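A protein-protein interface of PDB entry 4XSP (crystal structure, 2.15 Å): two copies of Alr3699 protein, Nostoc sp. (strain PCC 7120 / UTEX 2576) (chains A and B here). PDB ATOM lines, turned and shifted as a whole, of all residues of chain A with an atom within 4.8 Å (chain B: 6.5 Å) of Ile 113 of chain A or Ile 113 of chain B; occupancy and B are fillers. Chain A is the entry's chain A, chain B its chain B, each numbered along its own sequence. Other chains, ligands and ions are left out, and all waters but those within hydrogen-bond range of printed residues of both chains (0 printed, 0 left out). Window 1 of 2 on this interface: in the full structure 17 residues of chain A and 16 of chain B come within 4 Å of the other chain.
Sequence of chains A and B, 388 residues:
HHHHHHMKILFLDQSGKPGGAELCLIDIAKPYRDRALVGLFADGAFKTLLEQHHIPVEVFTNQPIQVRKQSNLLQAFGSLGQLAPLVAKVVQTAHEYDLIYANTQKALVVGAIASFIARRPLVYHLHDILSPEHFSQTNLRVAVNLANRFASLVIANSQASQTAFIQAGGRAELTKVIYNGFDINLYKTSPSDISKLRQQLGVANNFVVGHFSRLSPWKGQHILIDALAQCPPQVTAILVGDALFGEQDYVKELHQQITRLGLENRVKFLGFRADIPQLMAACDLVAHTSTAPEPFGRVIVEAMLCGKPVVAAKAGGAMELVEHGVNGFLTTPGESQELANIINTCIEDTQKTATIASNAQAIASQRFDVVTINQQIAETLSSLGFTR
Ile 113 of chain A touches its own counterpart, Ile 113 of chain B. Phe 116 of chain B touches its own counterpart, Phe 116 of chain A. Of the 4 pairs that touch across the chains among the printed residues, 2 have their exchanged pair printed and touching as well.
Among the printed residues, merely in contact across the chains: Phe 116 of chain A with Phe 116 of chain B (2.8 Å), Phe 116 of chain A with Phe 150 of chain B (3.8 Å), Phe 116 of chain A with Leu 146 of chain B (3.9 Å) and Ile 113 of chain A with Ile 113 of chain B (3.96 Å).
Ile 113 of chain A touches one residue of chain B. Of the printed residues of chain A, Ile 113 of chain B touches Ile 113 (3.96 Å). Of the printed residues of chain A, Leu 146 of chain B touches Phe 116. Of the printed residues of chain A, Phe 150 of chain B touches Phe 116 (3.8 Å). Of the printed residues of chain B, Phe 116 of chain A touches Phe 116, Leu 146 and Phe 150. Printed residues of chain A within 4 Å of Phe 116 of chain B: Phe 116 (2.8 Å). Val 109 of chain B touches none of the printed residues of chain A. Val 110 of chain A touches none of the printed residues of chain B.
Hydrophobic or aromatic side chains of chain A within 4 Å of the printed part of chain B: Ile 113 and Phe 116. Hydrophobic or aromatic side chains of chain B that line the printed part of chain A: Ile 113, Phe 116, Leu 146 and Phe 150. Along chain B the printed residues that touch a printed residue of chain A span positions 113 to 150. Among the printed residues, 4 pairs touch across the chains. Among the printed residues, no Asp or Glu carboxylate lies within 4 Å of a Lys or Arg side-chain nitrogen of the other chain.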
ATOM      1  N   VAL A  87     -21.221  21.772   2.462  1.00  0.00           N
ATOM      2  CA  VAL A  87     -20.460  22.996   2.683  1.00  0.00           C
ATOM      3  C   VAL A  87     -19.703  23.369   1.426  1.00  0.00           C
ATOM      4  O   VAL A  87     -19.676  24.536   1.024  1.00  0.00           O
ATOM      5  CB  VAL A  87     -19.499  22.833   3.873  1.00  0.00           C
ATOM      6  CG1 VAL A  87     -18.587  24.041   4.026  1.00  0.00           C
ATOM      7  CG2 VAL A  87     -20.306  22.586   5.150  1.00  0.00           C
ATOM      8  N   VAL A 109     -24.913  27.830  10.389  1.00  0.00           N
ATOM      9  CA  VAL A 109     -23.704  27.084  10.690  1.00  0.00           C
ATOM     10  C   VAL A 109     -22.952  26.888   9.394  1.00  0.00           C
ATOM     11  O   VAL A 109     -21.767  27.231   9.268  1.00  0.00           O
ATOM     12  CB  VAL A 109     -24.046  25.752  11.350  1.00  0.00           C
ATOM     13  CG1 VAL A 109     -22.770  24.951  11.539  1.00  0.00           C
ATOM     14  CG2 VAL A 109     -24.771  26.003  12.670  1.00  0.00           C
ATOM     15  N   VAL A 110     -23.670  26.406   8.395  1.00  0.00           N
ATOM     16  CA  VAL A 110     -23.093  26.224   7.069  1.00  0.00           C
ATOM     17  C   VAL A 110     -22.686  27.525   6.407  1.00  0.00           C
ATOM     18  O   VAL A 110     -21.645  27.598   5.731  1.00  0.00           O
ATOM     19  CB  VAL A 110     -24.082  25.472   6.165  1.00  0.00           C
ATOM     20  CG1 VAL A 110     -23.584  25.436   4.735  1.00  0.00           C
ATOM     21  CG2 VAL A 110     -24.308  24.082   6.715  1.00  0.00           C
ATOM     22  N   GLY A 111     -23.526  28.547   6.574  1.00  0.00           N
ATOM     23  CA  GLY A 111     -23.257  29.857   6.001  1.00  0.00           C
ATOM     24  C   GLY A 111     -22.014  30.505   6.581  1.00  0.00           C
ATOM     25  O   GLY A 111     -21.275  31.158   5.867  1.00  0.00           O
ATOM     26  N   ALA A 112     -21.797  30.344   7.880  1.00  0.00           N
ATOM     27  CA  ALA A 112     -20.608  30.914   8.528  1.00  0.00           C
ATOM     28  C   ALA A 112     -19.305  30.302   7.986  1.00  0.00           C
ATOM     29  O   ALA A 112     -18.347  31.004   7.611  1.00  0.00           O
ATOM     30  CB  ALA A 112     -20.715  30.717  10.029  1.00  0.00           C
ATOM     31  N   ILE A 113     -19.288  28.989   7.873  1.00  0.00           N
ATOM     32  CA  ILE A 113     -18.147  28.313   7.313  1.00  0.00           C
ATOM     33  C   ILE A 113     -17.938  28.726   5.893  1.00  0.00           C
ATOM     34  O   ILE A 113     -16.861  29.119   5.520  1.00  0.00           O
ATOM     35  CB  ILE A 113     -18.321  26.803   7.398  1.00  0.00           C
ATOM     36  CG1 ILE A 113     -18.372  26.389   8.850  1.00  0.00           C
ATOM     37  CG2 ILE A 113     -17.147  26.120   6.786  1.00  0.00           C
ATOM     38  CD1 ILE A 113     -19.319  25.285   9.156  1.00  0.00           C
ATOM     39  N   ALA A 114     -19.010  28.752   5.131  1.00  0.00           N
ATOM     40  CA  ALA A 114     -18.906  29.129   3.758  1.00  0.00           C
ATOM     41  C   ALA A 114     -18.415  30.535   3.640  1.00  0.00           C
ATOM     42  O   ALA A 114     -17.693  30.830   2.741  1.00  0.00           O
ATOM     43  CB  ALA A 114     -20.205  28.965   3.036  1.00  0.00           C
ATOM     44  N   SER A 115     -18.849  31.410   4.524  1.00  0.00           N
ATOM     45  CA  SER A 115     -18.421  32.779   4.459  1.00  0.00           C
ATOM     46  C   SER A 115     -16.915  32.977   4.660  1.00  0.00           C
ATOM     47  O   SER A 115     -16.309  33.699   3.911  1.00  0.00           O
ATOM     48  CB  SER A 115     -19.213  33.624   5.438  1.00  0.00           C
ATOM     49  OG  SER A 115     -18.588  33.746   6.665  1.00  0.00           O
ATOM     50  N   PHE A 116     -16.337  32.323   5.651  1.00  0.00           N
ATOM     51  CA  PHE A 116     -14.912  32.423   5.828  1.00  0.00           C
ATOM     52  C   PHE A 116     -14.127  31.791   4.690  1.00  0.00           C
ATOM     53  O   PHE A 116     -13.235  32.406   4.189  1.00  0.00           O
ATOM     54  CB  PHE A 116     -14.385  32.217   7.260  1.00  0.00           C
ATOM     55  CG  PHE A 116     -14.630  30.872   7.857  1.00  0.00           C
ATOM     56  CD1 PHE A 116     -13.877  29.777   7.476  1.00  0.00           C
ATOM     57  CD2 PHE A 116     -15.529  30.719   8.887  1.00  0.00           C
ATOM     58  CE1 PHE A 116     -14.061  28.552   8.071  1.00  0.00           C
ATOM     59  CE2 PHE A 116     -15.720  29.492   9.480  1.00  0.00           C
ATOM     60  CZ  PHE A 116     -14.984  28.407   9.074  1.00  0.00           C
ATOM     61  N   ILE A 117     -14.524  30.625   4.223  1.00  0.00           N
ATOM     62  CA  ILE A 117     -13.861  30.021   3.083  1.00  0.00           C
ATOM     63  C   ILE A 117     -14.015  30.726   1.744  1.00  0.00           C
ATOM     64  O   ILE A 117     -13.042  30.970   1.096  1.00  0.00           O
ATOM     65  CB  ILE A 117     -14.295  28.577   2.942  1.00  0.00           C
ATOM     66  CG1 ILE A 117     -14.111  27.895   4.265  1.00  0.00           C
ATOM     67  CG2 ILE A 117     -13.557  27.911   1.810  1.00  0.00           C
ATOM     68  CD1 ILE A 117     -13.988  26.404   4.196  1.00  0.00           C
ATOM     69  N   LEU B  80     -24.455  19.884  13.152  1.00  0.00           N
ATOM     70  CA  LEU B  80     -23.340  19.663  12.215  1.00  0.00           C
ATOM     71  C   LEU B  80     -23.058  18.153  11.966  1.00  0.00           C
ATOM     72  O   LEU B  80     -22.516  17.758  10.921  1.00  0.00           O
ATOM     73  CB  LEU B  80     -22.091  20.390  12.750  1.00  0.00           C
ATOM     74  CG  LEU B  80     -20.846  20.550  11.871  1.00  0.00           C
ATOM     75  CD1 LEU B  80     -21.123  21.293  10.567  1.00  0.00           C
ATOM     76  CD2 LEU B  80     -19.773  21.247  12.698  1.00  0.00           C
ATOM     77  N   VAL B  87     -16.416  16.546   9.808  1.00  0.00           N
ATOM     78  CA  VAL B  87     -16.105  17.754  10.610  1.00  0.00           C
ATOM     79  C   VAL B  87     -16.681  17.639  12.005  1.00  0.00           C
ATOM     80  O   VAL B  87     -16.016  17.961  12.993  1.00  0.00           O
ATOM     81  CB  VAL B  87     -16.648  19.048   9.951  1.00  0.00           C
ATOM     82  CG1 VAL B  87     -16.681  20.223  10.928  1.00  0.00           C
ATOM     83  CG2 VAL B  87     -15.822  19.408   8.736  1.00  0.00           C
ATOM     84  N   VAL B  91     -14.708  17.909  15.530  1.00  0.00           N
ATOM     85  CA  VAL B  91     -15.085  18.920  16.514  1.00  0.00           C
ATOM     86  C   VAL B  91     -15.347  18.302  17.854  1.00  0.00           C
ATOM     87  O   VAL B  91     -14.809  18.725  18.862  1.00  0.00           O
ATOM     88  CB  VAL B  91     -16.342  19.669  16.091  1.00  0.00           C
ATOM     89  CG1 VAL B  91     -17.054  20.287  17.292  1.00  0.00           C
ATOM     90  CG2 VAL B  91     -15.958  20.743  15.108  1.00  0.00           C
ATOM     91  N   LEU B 108      -5.629  20.563   7.859  1.00  0.00           N
ATOM     92  CA  LEU B 108      -5.699  22.006   8.082  1.00  0.00           C
ATOM     93  C   LEU B 108      -7.107  22.573   7.826  1.00  0.00           C
ATOM     94  O   LEU B 108      -7.649  23.284   8.663  1.00  0.00           O
ATOM     95  CB  LEU B 108      -4.698  22.747   7.193  1.00  0.00           C
ATOM     96  CG  LEU B 108      -4.879  24.268   7.349  1.00  0.00           C
ATOM     97  CD1 LEU B 108      -4.478  24.716   8.743  1.00  0.00           C
ATOM     98  CD2 LEU B 108      -4.145  25.042   6.283  1.00  0.00           C
ATOM     99  N   VAL B 109      -7.681  22.244   6.668  1.00  0.00           N
ATOM    100  CA  VAL B 109      -9.043  22.686   6.303  1.00  0.00           C
ATOM    101  C   VAL B 109      -9.999  22.254   7.371  1.00  0.00           C
ATOM    102  O   VAL B 109     -10.643  23.090   8.004  1.00  0.00           O
ATOM    103  CB  VAL B 109      -9.504  22.139   4.933  1.00  0.00           C
ATOM    104  CG1 VAL B 109     -10.994  22.388   4.721  1.00  0.00           C
ATOM    105  CG2 VAL B 109      -8.731  22.812   3.822  1.00  0.00           C
ATOM    106  N   VAL B 110     -10.051  20.951   7.617  1.00  0.00           N
ATOM    107  CA  VAL B 110     -10.892  20.439   8.677  1.00  0.00           C
ATOM    108  C   VAL B 110     -10.535  20.989  10.038  1.00  0.00           C
ATOM    109  O   VAL B 110     -11.431  21.322  10.826  1.00  0.00           O
ATOM    110  CB  VAL B 110     -10.868  18.906   8.735  1.00  0.00           C
ATOM    111  CG1 VAL B 110     -11.582  18.402   9.984  1.00  0.00           C
ATOM    112  CG2 VAL B 110     -11.506  18.328   7.488  1.00  0.00           C
ATOM    113  N   GLY B 111      -9.236  21.039  10.347  1.00  0.00           N
ATOM    114  CA  GLY B 111      -8.800  21.415  11.691  1.00  0.00           C
ATOM    115  C   GLY B 111      -9.134  22.846  12.051  1.00  0.00           C
ATOM    116  O   GLY B 111      -9.443  23.143  13.201  1.00  0.00           O
ATOM    117  N   ALA B 112      -9.026  23.742  11.073  1.00  0.00           N
ATOM    118  CA  ALA B 112      -9.412  25.151  11.243  1.00  0.00           C
ATOM    119  C   ALA B 112     -10.896  25.268  11.580  1.00  0.00           C
ATOM    120  O   ALA B 112     -11.287  25.985  12.516  1.00  0.00           O
ATOM    121  CB  ALA B 112      -9.059  25.952  10.000  1.00  0.00           C
ATOM    122  N   ILE B 113     -11.727  24.497  10.874  1.00  0.00           N
ATOM    123  CA  ILE B 113     -13.169  24.486  11.172  1.00  0.00           C
ATOM    124  C   ILE B 113     -13.383  24.026  12.591  1.00  0.00           C
ATOM    125  O   ILE B 113     -14.080  24.668  13.369  1.00  0.00           O
ATOM    126  CB  ILE B 113     -13.949  23.598  10.192  1.00  0.00           C
ATOM    127  CG1 ILE B 113     -13.859  24.194   8.798  1.00  0.00           C
ATOM    128  CG2 ILE B 113     -15.403  23.495  10.607  1.00  0.00           C
ATOM    129  CD1 ILE B 113     -14.495  23.333   7.728  1.00  0.00           C
ATOM    130  N   ALA B 114     -12.744  22.919  12.949  1.00  0.00           N
ATOM    131  CA  ALA B 114     -12.898  22.370  14.291  1.00  0.00           C
ATOM    132  C   ALA B 114     -12.314  23.291  15.364  1.00  0.00           C
ATOM    133  O   ALA B 114     -12.772  23.313  16.523  1.00  0.00           O
ATOM    134  CB  ALA B 114     -12.240  21.002  14.347  1.00  0.00           C
ATOM    135  N   SER B 115     -11.290  24.053  14.980  1.00  0.00           N
ATOM    136  CA  SER B 115     -10.585  24.879  15.931  1.00  0.00           C
ATOM    137  C   SER B 115     -11.464  25.959  16.572  1.00  0.00           C
ATOM    138  O   SER B 115     -11.486  26.107  17.818  1.00  0.00           O
ATOM    139  CB  SER B 115      -9.383  25.552  15.278  1.00  0.00           C
ATOM    140  OG  SER B 115      -8.732  26.352  16.244  1.00  0.00           O
ATOM    141  N   PHE B 116     -12.165  26.743  15.761  1.00  0.00           N
ATOM    142  CA  PHE B 116     -13.056  27.740  16.393  1.00  0.00           C
ATOM    143  C   PHE B 116     -14.303  27.128  17.057  1.00  0.00           C
ATOM    144  O   PHE B 116     -14.647  27.542  18.149  1.00  0.00           O
ATOM    145  CB  PHE B 116     -13.430  28.894  15.466  1.00  0.00           C
ATOM    146  CG  PHE B 116     -13.997  28.456  14.187  1.00  0.00           C
ATOM    147  CD1 PHE B 116     -15.330  28.109  14.105  1.00  0.00           C
ATOM    148  CD2 PHE B 116     -13.201  28.373  13.056  1.00  0.00           C
ATOM    149  CE1 PHE B 116     -15.875  27.691  12.909  1.00  0.00           C
ATOM    150  CE2 PHE B 116     -13.735  27.955  11.854  1.00  0.00           C
ATOM    151  CZ  PHE B 116     -15.082  27.606  11.789  1.00  0.00           C
ATOM    152  N   ILE B 117     -14.935  26.124  16.441  1.00  0.00           N
ATOM    153  CA  ILE B 117     -16.197  25.567  16.975  1.00  0.00           C
ATOM    154  C   ILE B 117     -15.924  24.905  18.289  1.00  0.00           C
ATOM    155  O   ILE B 117     -16.646  25.125  19.253  1.00  0.00           O
ATOM    156  CB  ILE B 117     -16.866  24.541  16.026  1.00  0.00           C
ATOM    157  CG1 ILE B 117     -17.159  25.175  14.664  1.00  0.00           C
ATOM    158  CG2 ILE B 117     -18.142  23.982  16.634  1.00  0.00           C
ATOM    159  CD1 ILE B 117     -17.877  24.262  13.676  1.00  0.00           C
ATOM    160  N   ALA B 118     -14.872  24.094  18.363  1.00  0.00           N
ATOM    161  CA  ALA B 118     -14.533  23.496  19.656  1.00  0.00           C
ATOM    162  C   ALA B 118     -13.804  24.479  20.532  1.00  0.00           C
ATOM    163  O   ALA B 118     -13.580  24.194  21.714  1.00  0.00           O
ATOM    164  CB  ALA B 118     -13.677  22.239  19.472  1.00  0.00           C
ATOM    165  N   LEU B 122      -4.957  25.954  17.186  1.00  0.00           N
ATOM    166  CA  LEU B 122      -4.589  25.165  16.030  1.00  0.00           C
ATOM    167  C   LEU B 122      -3.156  25.445  15.666  1.00  0.00           C
ATOM    168  O   LEU B 122      -2.720  26.618  15.631  1.00  0.00           O
ATOM    169  CB  LEU B 122      -5.474  25.518  14.830  1.00  0.00           C
ATOM    170  CG  LEU B 122      -5.131  24.857  13.497  1.00  0.00           C
ATOM    171  CD1 LEU B 122      -5.513  23.385  13.550  1.00  0.00           C
ATOM    172  CD2 LEU B 122      -5.839  25.566  12.349  1.00  0.00           C
ATOM    173  N   LEU B 146      -7.161  29.874   5.534  1.00  0.00           N
ATOM    174  CA  LEU B 146      -7.495  29.227   6.791  1.00  0.00           C
ATOM    175  C   LEU B 146      -6.359  29.316   7.812  1.00  0.00           C
ATOM    176  O   LEU B 146      -6.580  29.686   8.966  1.00  0.00           O
ATOM    177  CB  LEU B 146      -7.894  27.802   6.531  1.00  0.00           C
ATOM    178  CG  LEU B 146      -9.231  27.705   5.783  1.00  0.00           C
ATOM    179  CD1 LEU B 146      -9.671  26.259   5.627  1.00  0.00           C
ATOM    180  CD2 LEU B 146     -10.297  28.499   6.510  1.00  0.00           C
ATOM    181  N   PHE B 150      -6.768  31.140  11.275  1.00  0.00           N
ATOM    182  CA  PHE B 150      -7.038  30.281  12.419  1.00  0.00           C
ATOM    183  C   PHE B 150      -5.831  29.641  13.060  1.00  0.00           C
ATOM    184  O   PHE B 150      -5.928  29.207  14.187  1.00  0.00           O
ATOM    185  CB  PHE B 150      -8.020  29.213  12.002  1.00  0.00           C
ATOM    186  CG  PHE B 150      -9.326  29.778  11.555  1.00  0.00           C
ATOM    187  CD1 PHE B 150     -10.223  30.314  12.494  1.00  0.00           C
ATOM    188  CD2 PHE B 150      -9.658  29.816  10.204  1.00  0.00           C
ATOM    189  CE1 PHE B 150     -11.436  30.864  12.069  1.00  0.00           C
ATOM    190  CE2 PHE B 150     -10.866  30.356   9.787  1.00  0.00           C
ATOM    191  CZ  PHE B 150     -11.753  30.872  10.710  1.00  0.00           C
